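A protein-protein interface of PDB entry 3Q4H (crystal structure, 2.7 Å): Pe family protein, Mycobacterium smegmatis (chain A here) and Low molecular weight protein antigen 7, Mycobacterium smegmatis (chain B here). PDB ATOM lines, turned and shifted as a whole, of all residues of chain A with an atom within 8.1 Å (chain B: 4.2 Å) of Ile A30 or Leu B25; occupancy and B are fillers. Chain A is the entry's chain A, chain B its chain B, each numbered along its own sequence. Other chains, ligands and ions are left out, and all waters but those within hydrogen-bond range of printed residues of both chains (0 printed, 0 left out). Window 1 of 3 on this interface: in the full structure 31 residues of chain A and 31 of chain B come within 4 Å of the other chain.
Of chain A, only Met A26 (3.5 Å), Thr A29 (3.6 Å) and Ile A30 (3.8 Å) come within 4 Å of Leu B25.
Of the printed residues of chain B, Ala A33 touches Tyr B21 (3.7 Å).
Of the printed residues of chain B, Ser A63 touches Leu B65.
Printed residues of chain B within 4 Å of Thr A29: Leu B25.
Of the printed residues of chain A, Val B28 touches Met A26 (3.2 Å).
Of the printed residues of chain B, Phe A59 touches Leu B65.
Val A66 touches none of the printed residues of chain B.
Met A26 touches Leu B25 (CE to O, 3.5 Å).
Met A26 touches Val B28 (CE to C, 3.2 Å).
CE of Met A26 touches N of Gly B29, 2.8 Å away.
Thr A29 touches Leu B25.
Ile A30 touches Leu B25 (CG1 to CD2, 3.8 Å).
Gln A32 touches Tyr B21 (NE2 to OH, 3.5 Å).
Tyr B21 touches Ala A36.
CE1 of Phe A59 touches CD1 of Leu B65, at 3.6 Å.
CG1 of Val A62 touches CB of Leu B65, 3.6 Å away.
Ser A63 touches Leu B65 (OG to CD1, 3.5 Å).
OG1 of Thr A29 lies within hydrogen-bond range of O of Leu A25, at 2.8 Å.
O of Phe A59 lies within hydrogen-bond range of OG of Ser A63, 3.0 Å away.
O of Ser A63 lies within hydrogen-bond range of ND2 of Asn A67 (2.9 Å).
Hydrophobic or aromatic side chains of chain A within 4 Å of the printed part of chain B: Met A26, Ile A30, Ala A33, Ala A36, Phe A59 and Val A62.
Printed residues of chain B that touch a printed residue of chain A: Tyr B21, Leu B25, Val B28, Gly B29 and Leu B65.
Hydrophobic or aromatic side chains of chain B that line the printed part of chain A: Tyr B21, Leu B25, Val B28 and Leu B65.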
ATOM      1  N   ALA A  23      15.373 -27.877 -27.672  1.00  0.00           N
ATOM      2  CA  ALA A  23      13.957 -27.623 -27.840  1.00  0.00           C
ATOM      3  C   ALA A  23      13.194 -28.591 -26.943  1.00  0.00           C
ATOM      4  O   ALA A  23      12.342 -28.178 -26.152  1.00  0.00           O
ATOM      5  CB  ALA A  23      13.546 -27.774 -29.291  1.00  0.00           C
ATOM      6  N   ALA A  24      13.525 -29.875 -27.025  1.00  0.00           N
ATOM      7  CA  ALA A  24      12.836 -30.867 -26.202  1.00  0.00           C
ATOM      8  C   ALA A  24      13.064 -30.581 -24.724  1.00  0.00           C
ATOM      9  O   ALA A  24      12.163 -30.748 -23.921  1.00  0.00           O
ATOM     10  CB  ALA A  24      13.289 -32.253 -26.544  1.00  0.00           C
ATOM     11  N   LEU A  25      14.255 -30.110 -24.373  1.00  0.00           N
ATOM     12  CA  LEU A  25      14.580 -29.847 -22.975  1.00  0.00           C
ATOM     13  C   LEU A  25      13.836 -28.632 -22.410  1.00  0.00           C
ATOM     14  O   LEU A  25      13.508 -28.603 -21.218  1.00  0.00           O
ATOM     15  CB  LEU A  25      16.097 -29.719 -22.788  1.00  0.00           C
ATOM     16  CG  LEU A  25      16.863 -31.051 -22.891  1.00  0.00           C
ATOM     17  CD1 LEU A  25      18.356 -30.861 -22.658  1.00  0.00           C
ATOM     18  CD2 LEU A  25      16.305 -32.078 -21.918  1.00  0.00           C
ATOM     19  N   MET A  26      13.548 -27.650 -23.262  1.00  0.00           N
ATOM     20  CA  MET A  26      12.644 -26.565 -22.886  1.00  0.00           C
ATOM     21  C   MET A  26      11.243 -27.116 -22.556  1.00  0.00           C
ATOM     22  O   MET A  26      10.728 -26.877 -21.470  1.00  0.00           O
ATOM     23  CB  MET A  26      12.554 -25.524 -23.997  1.00  0.00           C
ATOM     24  CG  MET A  26      11.564 -24.384 -23.731  1.00  0.00           C
ATOM     25  SD  MET A  26      11.976 -23.242 -22.176  1.00  0.00           S
ATOM     26  CE  MET A  26      13.570 -22.380 -22.849  1.00  0.00           C
ATOM     27  N   ARG A  27      10.644 -27.868 -23.480  1.00  0.00           N
ATOM     28  CA  ARG A  27       9.346 -28.493 -23.235  1.00  0.00           C
ATOM     29  C   ARG A  27       9.341 -29.251 -21.904  1.00  0.00           C
ATOM     30  O   ARG A  27       8.332 -29.281 -21.200  1.00  0.00           O
ATOM     31  CB  ARG A  27       8.989 -29.486 -24.342  1.00  0.00           C
ATOM     32  CG  ARG A  27       8.891 -28.928 -25.757  1.00  0.00           C
ATOM     33  CD  ARG A  27       8.323 -29.982 -26.696  1.00  0.00           C
ATOM     34  NE  ARG A  27       8.789 -29.830 -28.075  1.00  0.00           N
ATOM     35  CZ  ARG A  27       8.172 -29.122 -29.018  1.00  0.00           C
ATOM     36  NH1 ARG A  27       7.059 -28.442 -28.753  1.00  0.00           N
ATOM     37  NH2 ARG A  27       8.681 -29.073 -30.241  1.00  0.00           N
ATOM     38  N   SER A  28      10.471 -29.883 -21.590  1.00  0.00           N
ATOM     39  CA  SER A  28      10.644 -30.631 -20.345  1.00  0.00           C
ATOM     40  C   SER A  28      10.698 -29.708 -19.124  1.00  0.00           C
ATOM     41  O   SER A  28      10.083 -29.983 -18.101  1.00  0.00           O
ATOM     42  CB  SER A  28      11.924 -31.471 -20.419  1.00  0.00           C
ATOM     43  OG  SER A  28      12.031 -32.335 -19.300  1.00  0.00           O
ATOM     44  N   THR A  29      11.450 -28.616 -19.247  1.00  0.00           N
ATOM     45  CA  THR A  29      11.541 -27.606 -18.200  1.00  0.00           C
ATOM     46  C   THR A  29      10.203 -26.947 -17.915  1.00  0.00           C
ATOM     47  O   THR A  29       9.861 -26.751 -16.754  1.00  0.00           O
ATOM     48  CB  THR A  29      12.525 -26.529 -18.597  1.00  0.00           C
ATOM     49  OG1 THR A  29      13.803 -27.139 -18.808  1.00  0.00           O
ATOM     50  CG2 THR A  29      12.631 -25.451 -17.515  1.00  0.00           C
ATOM     51  N   ILE A  30       9.459 -26.602 -18.968  1.00  0.00           N
ATOM     52  CA  ILE A  30       8.115 -26.064 -18.825  1.00  0.00           C
ATOM     53  C   ILE A  30       7.223 -27.025 -18.033  1.00  0.00           C
ATOM     54  O   ILE A  30       6.472 -26.593 -17.160  1.00  0.00           O
ATOM     55  CB  ILE A  30       7.455 -25.780 -20.209  1.00  0.00           C
ATOM     56  CG1 ILE A  30       8.103 -24.567 -20.872  1.00  0.00           C
ATOM     57  CG2 ILE A  30       5.953 -25.508 -20.073  1.00  0.00           C
ATOM     58  CD1 ILE A  30       7.639 -24.319 -22.279  1.00  0.00           C
ATOM     59  N   ALA A  31       7.320 -28.322 -18.347  1.00  0.00           N
ATOM     60  CA  ALA A  31       6.515 -29.370 -17.703  1.00  0.00           C
ATOM     61  C   ALA A  31       6.877 -29.567 -16.229  1.00  0.00           C
ATOM     62  O   ALA A  31       5.996 -29.709 -15.375  1.00  0.00           O
ATOM     63  CB  ALA A  31       6.660 -30.665 -18.452  1.00  0.00           C
ATOM     64  N   GLN A  32       8.171 -29.568 -15.931  1.00  0.00           N
ATOM     65  CA  GLN A  32       8.626 -29.625 -14.540  1.00  0.00           C
ATOM     66  C   GLN A  32       8.256 -28.368 -13.747  1.00  0.00           C
ATOM     67  O   GLN A  32       8.025 -28.434 -12.549  1.00  0.00           O
ATOM     68  CB  GLN A  32      10.143 -29.843 -14.477  1.00  0.00           C
ATOM     69  CG  GLN A  32      10.588 -31.205 -14.978  1.00  0.00           C
ATOM     70  CD  GLN A  32      12.051 -31.475 -14.682  1.00  0.00           C
ATOM     71  OE1 GLN A  32      12.868 -31.636 -15.598  1.00  0.00           O
ATOM     72  NE2 GLN A  32      12.397 -31.515 -13.397  1.00  0.00           N
ATOM     73  N   ALA A  33       8.215 -27.220 -14.412  1.00  0.00           N
ATOM     74  CA  ALA A  33       7.824 -25.982 -13.746  1.00  0.00           C
ATOM     75  C   ALA A  33       6.340 -26.019 -13.402  1.00  0.00           C
ATOM     76  O   ALA A  33       5.920 -25.496 -12.373  1.00  0.00           O
ATOM     77  CB  ALA A  33       8.144 -24.785 -14.617  1.00  0.00           C
ATOM     78  N   GLU A  34       5.561 -26.658 -14.266  1.00  0.00           N
ATOM     79  CA  GLU A  34       4.116 -26.787 -14.092  1.00  0.00           C
ATOM     80  C   GLU A  34       3.781 -27.682 -12.892  1.00  0.00           C
ATOM     81  O   GLU A  34       2.909 -27.353 -12.098  1.00  0.00           O
ATOM     82  CB  GLU A  34       3.499 -27.325 -15.393  1.00  0.00           C
ATOM     83  CG  GLU A  34       2.029 -27.732 -15.325  1.00  0.00           C
ATOM     84  CD  GLU A  34       1.063 -26.571 -15.349  1.00  0.00           C
ATOM     85  OE1 GLU A  34       1.505 -25.403 -15.335  1.00  0.00           O
ATOM     86  OE2 GLU A  34      -0.162 -26.836 -15.385  1.00  0.00           O
ATOM     87  N   GLN A  35       4.487 -28.802 -12.766  1.00  0.00           N
ATOM     88  CA  GLN A  35       4.326 -29.706 -11.623  1.00  0.00           C
ATOM     89  C   GLN A  35       4.613 -29.004 -10.305  1.00  0.00           C
ATOM     90  O   GLN A  35       3.888 -29.179  -9.331  1.00  0.00           O
ATOM     91  CB  GLN A  35       5.262 -30.905 -11.743  1.00  0.00           C
ATOM     92  CG  GLN A  35       4.945 -31.851 -12.883  1.00  0.00           C
ATOM     93  CD  GLN A  35       5.795 -33.123 -12.851  1.00  0.00           C
ATOM     94  OE1 GLN A  35       5.763 -33.875 -11.872  1.00  0.00           O
ATOM     95  NE2 GLN A  35       6.545 -33.371 -13.922  1.00  0.00           N
ATOM     96  N   ALA A  36       5.683 -28.221 -10.278  1.00  0.00           N
ATOM     97  CA  ALA A  36       6.033 -27.440  -9.101  1.00  0.00           C
ATOM     98  C   ALA A  36       4.987 -26.366  -8.801  1.00  0.00           C
ATOM     99  O   ALA A  36       4.763 -26.038  -7.646  1.00  0.00           O
ATOM    100  CB  ALA A  36       7.398 -26.812  -9.280  1.00  0.00           C
ATOM    101  N   ALA A  37       4.352 -25.828  -9.839  1.00  0.00           N
ATOM    102  CA  ALA A  37       3.269 -24.855  -9.682  1.00  0.00           C
ATOM    103  C   ALA A  37       1.978 -25.479  -9.124  1.00  0.00           C
ATOM    104  O   ALA A  37       1.399 -24.961  -8.168  1.00  0.00           O
ATOM    105  CB  ALA A  37       2.990 -24.183 -11.011  1.00  0.00           C
ATOM    106  N   PHE A  59      -0.028 -19.013 -17.796  1.00  0.00           N
ATOM    107  CA  PHE A  59       1.176 -19.788 -18.022  1.00  0.00           C
ATOM    108  C   PHE A  59       0.899 -21.000 -18.916  1.00  0.00           C
ATOM    109  O   PHE A  59       1.659 -21.283 -19.848  1.00  0.00           O
ATOM    110  CB  PHE A  59       1.753 -20.238 -16.692  1.00  0.00           C
ATOM    111  CG  PHE A  59       2.941 -21.136 -16.824  1.00  0.00           C
ATOM    112  CD1 PHE A  59       4.193 -20.612 -17.098  1.00  0.00           C
ATOM    113  CD2 PHE A  59       2.812 -22.506 -16.661  1.00  0.00           C
ATOM    114  CE1 PHE A  59       5.289 -21.435 -17.214  1.00  0.00           C
ATOM    115  CE2 PHE A  59       3.905 -23.332 -16.774  1.00  0.00           C
ATOM    116  CZ  PHE A  59       5.147 -22.796 -17.056  1.00  0.00           C
ATOM    117  N   VAL A  60      -0.189 -21.711 -18.632  1.00  0.00           N
ATOM    118  CA  VAL A  60      -0.588 -22.852 -19.458  1.00  0.00           C
ATOM    119  C   VAL A  60      -0.878 -22.426 -20.901  1.00  0.00           C
ATOM    120  O   VAL A  60      -0.553 -23.163 -21.827  1.00  0.00           O
ATOM    121  CB  VAL A  60      -1.798 -23.625 -18.843  1.00  0.00           C
ATOM    122  CG1 VAL A  60      -2.398 -24.608 -19.834  1.00  0.00           C
ATOM    123  CG2 VAL A  60      -1.358 -24.354 -17.589  1.00  0.00           C
ATOM    124  N   VAL A  62       0.560 -19.740 -22.551  1.00  0.00           N
ATOM    125  CA  VAL A  62       1.782 -19.311 -23.213  1.00  0.00           C
ATOM    126  C   VAL A  62       2.694 -20.507 -23.537  1.00  0.00           C
ATOM    127  O   VAL A  62       3.366 -20.498 -24.574  1.00  0.00           O
ATOM    128  CB  VAL A  62       2.525 -18.251 -22.380  1.00  0.00           C
ATOM    129  CG1 VAL A  62       3.793 -17.801 -23.076  1.00  0.00           C
ATOM    130  CG2 VAL A  62       1.628 -17.069 -22.130  1.00  0.00           C
ATOM    131  N   SER A  63       2.712 -21.525 -22.664  1.00  0.00           N
ATOM    132  CA  SER A  63       3.408 -22.791 -22.958  1.00  0.00           C
ATOM    133  C   SER A  63       2.949 -23.385 -24.270  1.00  0.00           C
ATOM    134  O   SER A  63       3.770 -23.839 -25.066  1.00  0.00           O
ATOM    135  CB  SER A  63       3.148 -23.832 -21.886  1.00  0.00           C
ATOM    136  OG  SER A  63       3.685 -23.408 -20.660  1.00  0.00           O
ATOM    137  N   ALA A  64       1.631 -23.391 -24.475  1.00  0.00           N
ATOM    138  CA  ALA A  64       1.048 -23.840 -25.734  1.00  0.00           C
ATOM    139  C   ALA A  64       1.656 -23.087 -26.919  1.00  0.00           C
ATOM    140  O   ALA A  64       2.036 -23.703 -27.912  1.00  0.00           O
ATOM    141  CB  ALA A  64      -0.462 -23.665 -25.712  1.00  0.00           C
ATOM    142  N   LYS A  65       1.764 -21.765 -26.807  1.00  0.00           N
ATOM    143  CA  LYS A  65       2.305 -20.950 -27.892  1.00  0.00           C
ATOM    144  C   LYS A  65       3.800 -21.232 -28.090  1.00  0.00           C
ATOM    145  O   LYS A  65       4.275 -21.331 -29.227  1.00  0.00           O
ATOM    146  CB  LYS A  65       2.056 -19.458 -27.631  1.00  0.00           C
ATOM    147  N   VAL A  66       4.528 -21.373 -26.983  1.00  0.00           N
ATOM    148  CA  VAL A  66       5.954 -21.679 -27.026  1.00  0.00           C
ATOM    149  C   VAL A  66       6.198 -23.070 -27.594  1.00  0.00           C
ATOM    150  O   VAL A  66       7.153 -23.292 -28.343  1.00  0.00           O
ATOM    151  CB  VAL A  66       6.592 -21.574 -25.633  1.00  0.00           C
ATOM    152  CG1 VAL A  66       7.940 -22.256 -25.604  1.00  0.00           C
ATOM    153  CG2 VAL A  66       6.723 -20.118 -25.228  1.00  0.00           C
ATOM    154  N   ASN A  67       5.336 -24.010 -27.243  1.00  0.00           N
ATOM    155  CA  ASN A  67       5.389 -25.323 -27.863  1.00  0.00           C
ATOM    156  C   ASN A  67       5.101 -25.228 -29.352  1.00  0.00           C
ATOM    157  O   ASN A  67       5.803 -25.843 -30.150  1.00  0.00           O
ATOM    158  CB  ASN A  67       4.452 -26.308 -27.162  1.00  0.00           C
ATOM    159  CG  ASN A  67       5.107 -26.956 -25.965  1.00  0.00           C
ATOM    160  OD1 ASN A  67       5.949 -27.836 -26.122  1.00  0.00           O
ATOM    161  ND2 ASN A  67       4.753 -26.509 -24.770  1.00  0.00           N
ATOM    162  N   LEU A  70       8.277 -23.838 -30.910  1.00  0.00           N
ATOM    163  CA  LEU A  70       9.325 -24.850 -30.989  1.00  0.00           C
ATOM    164  C   LEU A  70       9.024 -25.828 -32.128  1.00  0.00           C
ATOM    165  O   LEU A  70       9.934 -26.249 -32.845  1.00  0.00           O
ATOM    166  CB  LEU A  70       9.462 -25.604 -29.669  1.00  0.00           C
ATOM    167  CG  LEU A  70      10.012 -24.822 -28.468  1.00  0.00           C
ATOM    168  CD1 LEU A  70       9.897 -25.640 -27.158  1.00  0.00           C
ATOM    169  CD2 LEU A  70      11.458 -24.399 -28.714  1.00  0.00           C
ATOM    170  N   TYR B  21      12.803 -22.628 -11.244  1.00  0.00           N
ATOM    171  CA  TYR B  21      12.251 -22.842 -12.579  1.00  0.00           C
ATOM    172  C   TYR B  21      12.110 -21.542 -13.362  1.00  0.00           C
ATOM    173  O   TYR B  21      12.279 -21.537 -14.583  1.00  0.00           O
ATOM    174  CB  TYR B  21      10.913 -23.591 -12.498  1.00  0.00           C
ATOM    175  CG  TYR B  21      11.084 -25.035 -12.096  1.00  0.00           C
ATOM    176  CD1 TYR B  21      11.702 -25.938 -12.949  1.00  0.00           C
ATOM    177  CD2 TYR B  21      10.669 -25.491 -10.854  1.00  0.00           C
ATOM    178  CE1 TYR B  21      11.883 -27.268 -12.588  1.00  0.00           C
ATOM    179  CE2 TYR B  21      10.853 -26.815 -10.480  1.00  0.00           C
ATOM    180  CZ  TYR B  21      11.461 -27.700 -11.356  1.00  0.00           C
ATOM    181  OH  TYR B  21      11.653 -29.020 -11.003  1.00  0.00           O
ATOM    182  N   SER B  22      11.814 -20.444 -12.666  1.00  0.00           N
ATOM    183  CA  SER B  22      11.852 -19.111 -13.272  1.00  0.00           C
ATOM    184  C   SER B  22      13.207 -18.844 -13.918  1.00  0.00           C
ATOM    185  O   SER B  22      13.279 -18.414 -15.066  1.00  0.00           O
ATOM    186  CB  SER B  22      11.579 -18.037 -12.224  1.00  0.00           C
ATOM    187  OG  SER B  22      10.351 -18.267 -11.554  1.00  0.00           O
ATOM    188  N   GLY B  23      14.281 -19.106 -13.174  1.00  0.00           N
ATOM    189  CA  GLY B  23      15.636 -18.916 -13.669  1.00  0.00           C
ATOM    190  C   GLY B  23      15.942 -19.890 -14.784  1.00  0.00           C
ATOM    191  O   GLY B  23      16.587 -19.532 -15.777  1.00  0.00           O
ATOM    192  N   ALA B  24      15.470 -21.128 -14.619  1.00  0.00           N
ATOM    193  CA  ALA B  24      15.670 -22.172 -15.620  1.00  0.00           C
ATOM    194  C   ALA B  24      14.990 -21.813 -16.950  1.00  0.00           C
ATOM    195  O   ALA B  24      15.634 -21.806 -18.004  1.00  0.00           O
ATOM    196  CB  ALA B  24      15.163 -23.507 -15.092  1.00  0.00           C
ATOM    197  N   LEU B  25      13.700 -21.490 -16.894  1.00  0.00           N
ATOM    198  CA  LEU B  25      12.938 -21.123 -18.107  1.00  0.00           C
ATOM    199  C   LEU B  25      13.629 -20.023 -18.912  1.00  0.00           C
ATOM    200  O   LEU B  25      13.771 -20.124 -20.129  1.00  0.00           O
ATOM    201  CB  LEU B  25      11.510 -20.703 -17.749  1.00  0.00           C
ATOM    202  CG  LEU B  25      10.608 -21.860 -17.282  1.00  0.00           C
ATOM    203  CD1 LEU B  25       9.294 -21.340 -16.718  1.00  0.00           C
ATOM    204  CD2 LEU B  25      10.357 -22.863 -18.398  1.00  0.00           C
ATOM    205  N   HIS B  26      14.086 -18.994 -18.216  1.00  0.00           N
ATOM    206  CA  HIS B  26      14.764 -17.868 -18.846  1.00  0.00           C
ATOM    207  C   HIS B  26      16.055 -18.332 -19.537  1.00  0.00           C
ATOM    208  O   HIS B  26      16.211 -18.178 -20.749  1.00  0.00           O
ATOM    209  CB  HIS B  26      15.053 -16.809 -17.778  1.00  0.00           C
ATOM    210  CG  HIS B  26      15.727 -15.578 -18.294  1.00  0.00           C
ATOM    211  ND1 HIS B  26      15.034 -14.525 -18.851  1.00  0.00           N
ATOM    212  CD2 HIS B  26      17.030 -15.214 -18.299  1.00  0.00           C
ATOM    213  CE1 HIS B  26      15.884 -13.575 -19.195  1.00  0.00           C
ATOM    214  NE2 HIS B  26      17.102 -13.968 -18.875  1.00  0.00           N
ATOM    215  N   ALA B  27      16.953 -18.937 -18.760  1.00  0.00           N
ATOM    216  CA  ALA B  27      18.272 -19.339 -19.237  1.00  0.00           C
ATOM    217  C   ALA B  27      18.217 -20.133 -20.542  1.00  0.00           C
ATOM    218  O   ALA B  27      18.922 -19.797 -21.504  1.00  0.00           O
ATOM    219  CB  ALA B  27      19.003 -20.136 -18.155  1.00  0.00           C
ATOM    220  N   VAL B  28      17.377 -21.169 -20.568  1.00  0.00           N
ATOM    221  CA  VAL B  28      17.269 -22.064 -21.722  1.00  0.00           C
ATOM    222  C   VAL B  28      16.601 -21.353 -22.913  1.00  0.00           C
ATOM    223  O   VAL B  28      16.937 -21.615 -24.073  1.00  0.00           O
ATOM    224  CB  VAL B  28      16.476 -23.347 -21.373  1.00  0.00           C
ATOM    225  CG1 VAL B  28      16.333 -24.246 -22.588  1.00  0.00           C
ATOM    226  CG2 VAL B  28      17.146 -24.111 -20.242  1.00  0.00           C
ATOM    227  N   GLY B  29      15.657 -20.459 -22.623  1.00  0.00           N
ATOM    228  CA  GLY B  29      14.994 -19.699 -23.669  1.00  0.00           C
ATOM    229  C   GLY B  29      15.989 -18.787 -24.344  1.00  0.00           C
ATOM    230  O   GLY B  29      16.011 -18.675 -25.570  1.00  0.00           O
ATOM    231  N   MET B  62       8.831 -15.787 -24.772  1.00  0.00           N
ATOM    232  CA  MET B  62       9.629 -16.225 -23.623  1.00  0.00           C
ATOM    233  C   MET B  62       9.545 -15.246 -22.448  1.00  0.00           C
ATOM    234  O   MET B  62       9.687 -15.649 -21.298  1.00  0.00           O
ATOM    235  CB  MET B  62      11.096 -16.462 -24.021  1.00  0.00           C
ATOM    236  CG  MET B  62      11.359 -17.817 -24.670  1.00  0.00           C
ATOM    237  SD  MET B  62      10.714 -19.361 -23.622  1.00  0.00           S
ATOM    238  CE  MET B  62      11.464 -18.884 -21.870  1.00  0.00           C
ATOM    239  N   LEU B  65       6.003 -15.844 -20.782  1.00  0.00           N
ATOM    240  CA  LEU B  65       5.981 -17.154 -20.102  1.00  0.00           C
ATOM    241  C   LEU B  65       6.656 -17.097 -18.737  1.00  0.00           C
ATOM    242  O   LEU B  65       6.091 -17.540 -17.729  1.00  0.00           O
ATOM    243  CB  LEU B  65       6.668 -18.225 -20.948  1.00  0.00           C
ATOM    244  CG  LEU B  65       6.633 -19.649 -20.381  1.00  0.00           C
ATOM    245  CD1 LEU B  65       5.302 -20.319 -20.654  1.00  0.00           C
ATOM    246  CD2 LEU B  65       7.765 -20.464 -20.955  1.00  0.00           C
ATOM    247  N   VAL B  66       7.871 -16.560 -18.713  1.00  0.00           N
ATOM    248  CA  VAL B  66       8.592 -16.349 -17.460  1.00  0.00           C
ATOM    249  C   VAL B  66       7.855 -15.375 -16.527  1.00  0.00           C
ATOM    250  O   VAL B  66       7.819 -15.590 -15.325  1.00  0.00           O
ATOM    251  CB  VAL B  66      10.016 -15.846 -17.727  1.00  0.00           C
ATOM    252  CG1 VAL B  66      10.704 -15.442 -16.432  1.00  0.00           C
ATOM    253  CG2 VAL B  66      10.813 -16.925 -18.422  1.00  0.00           C
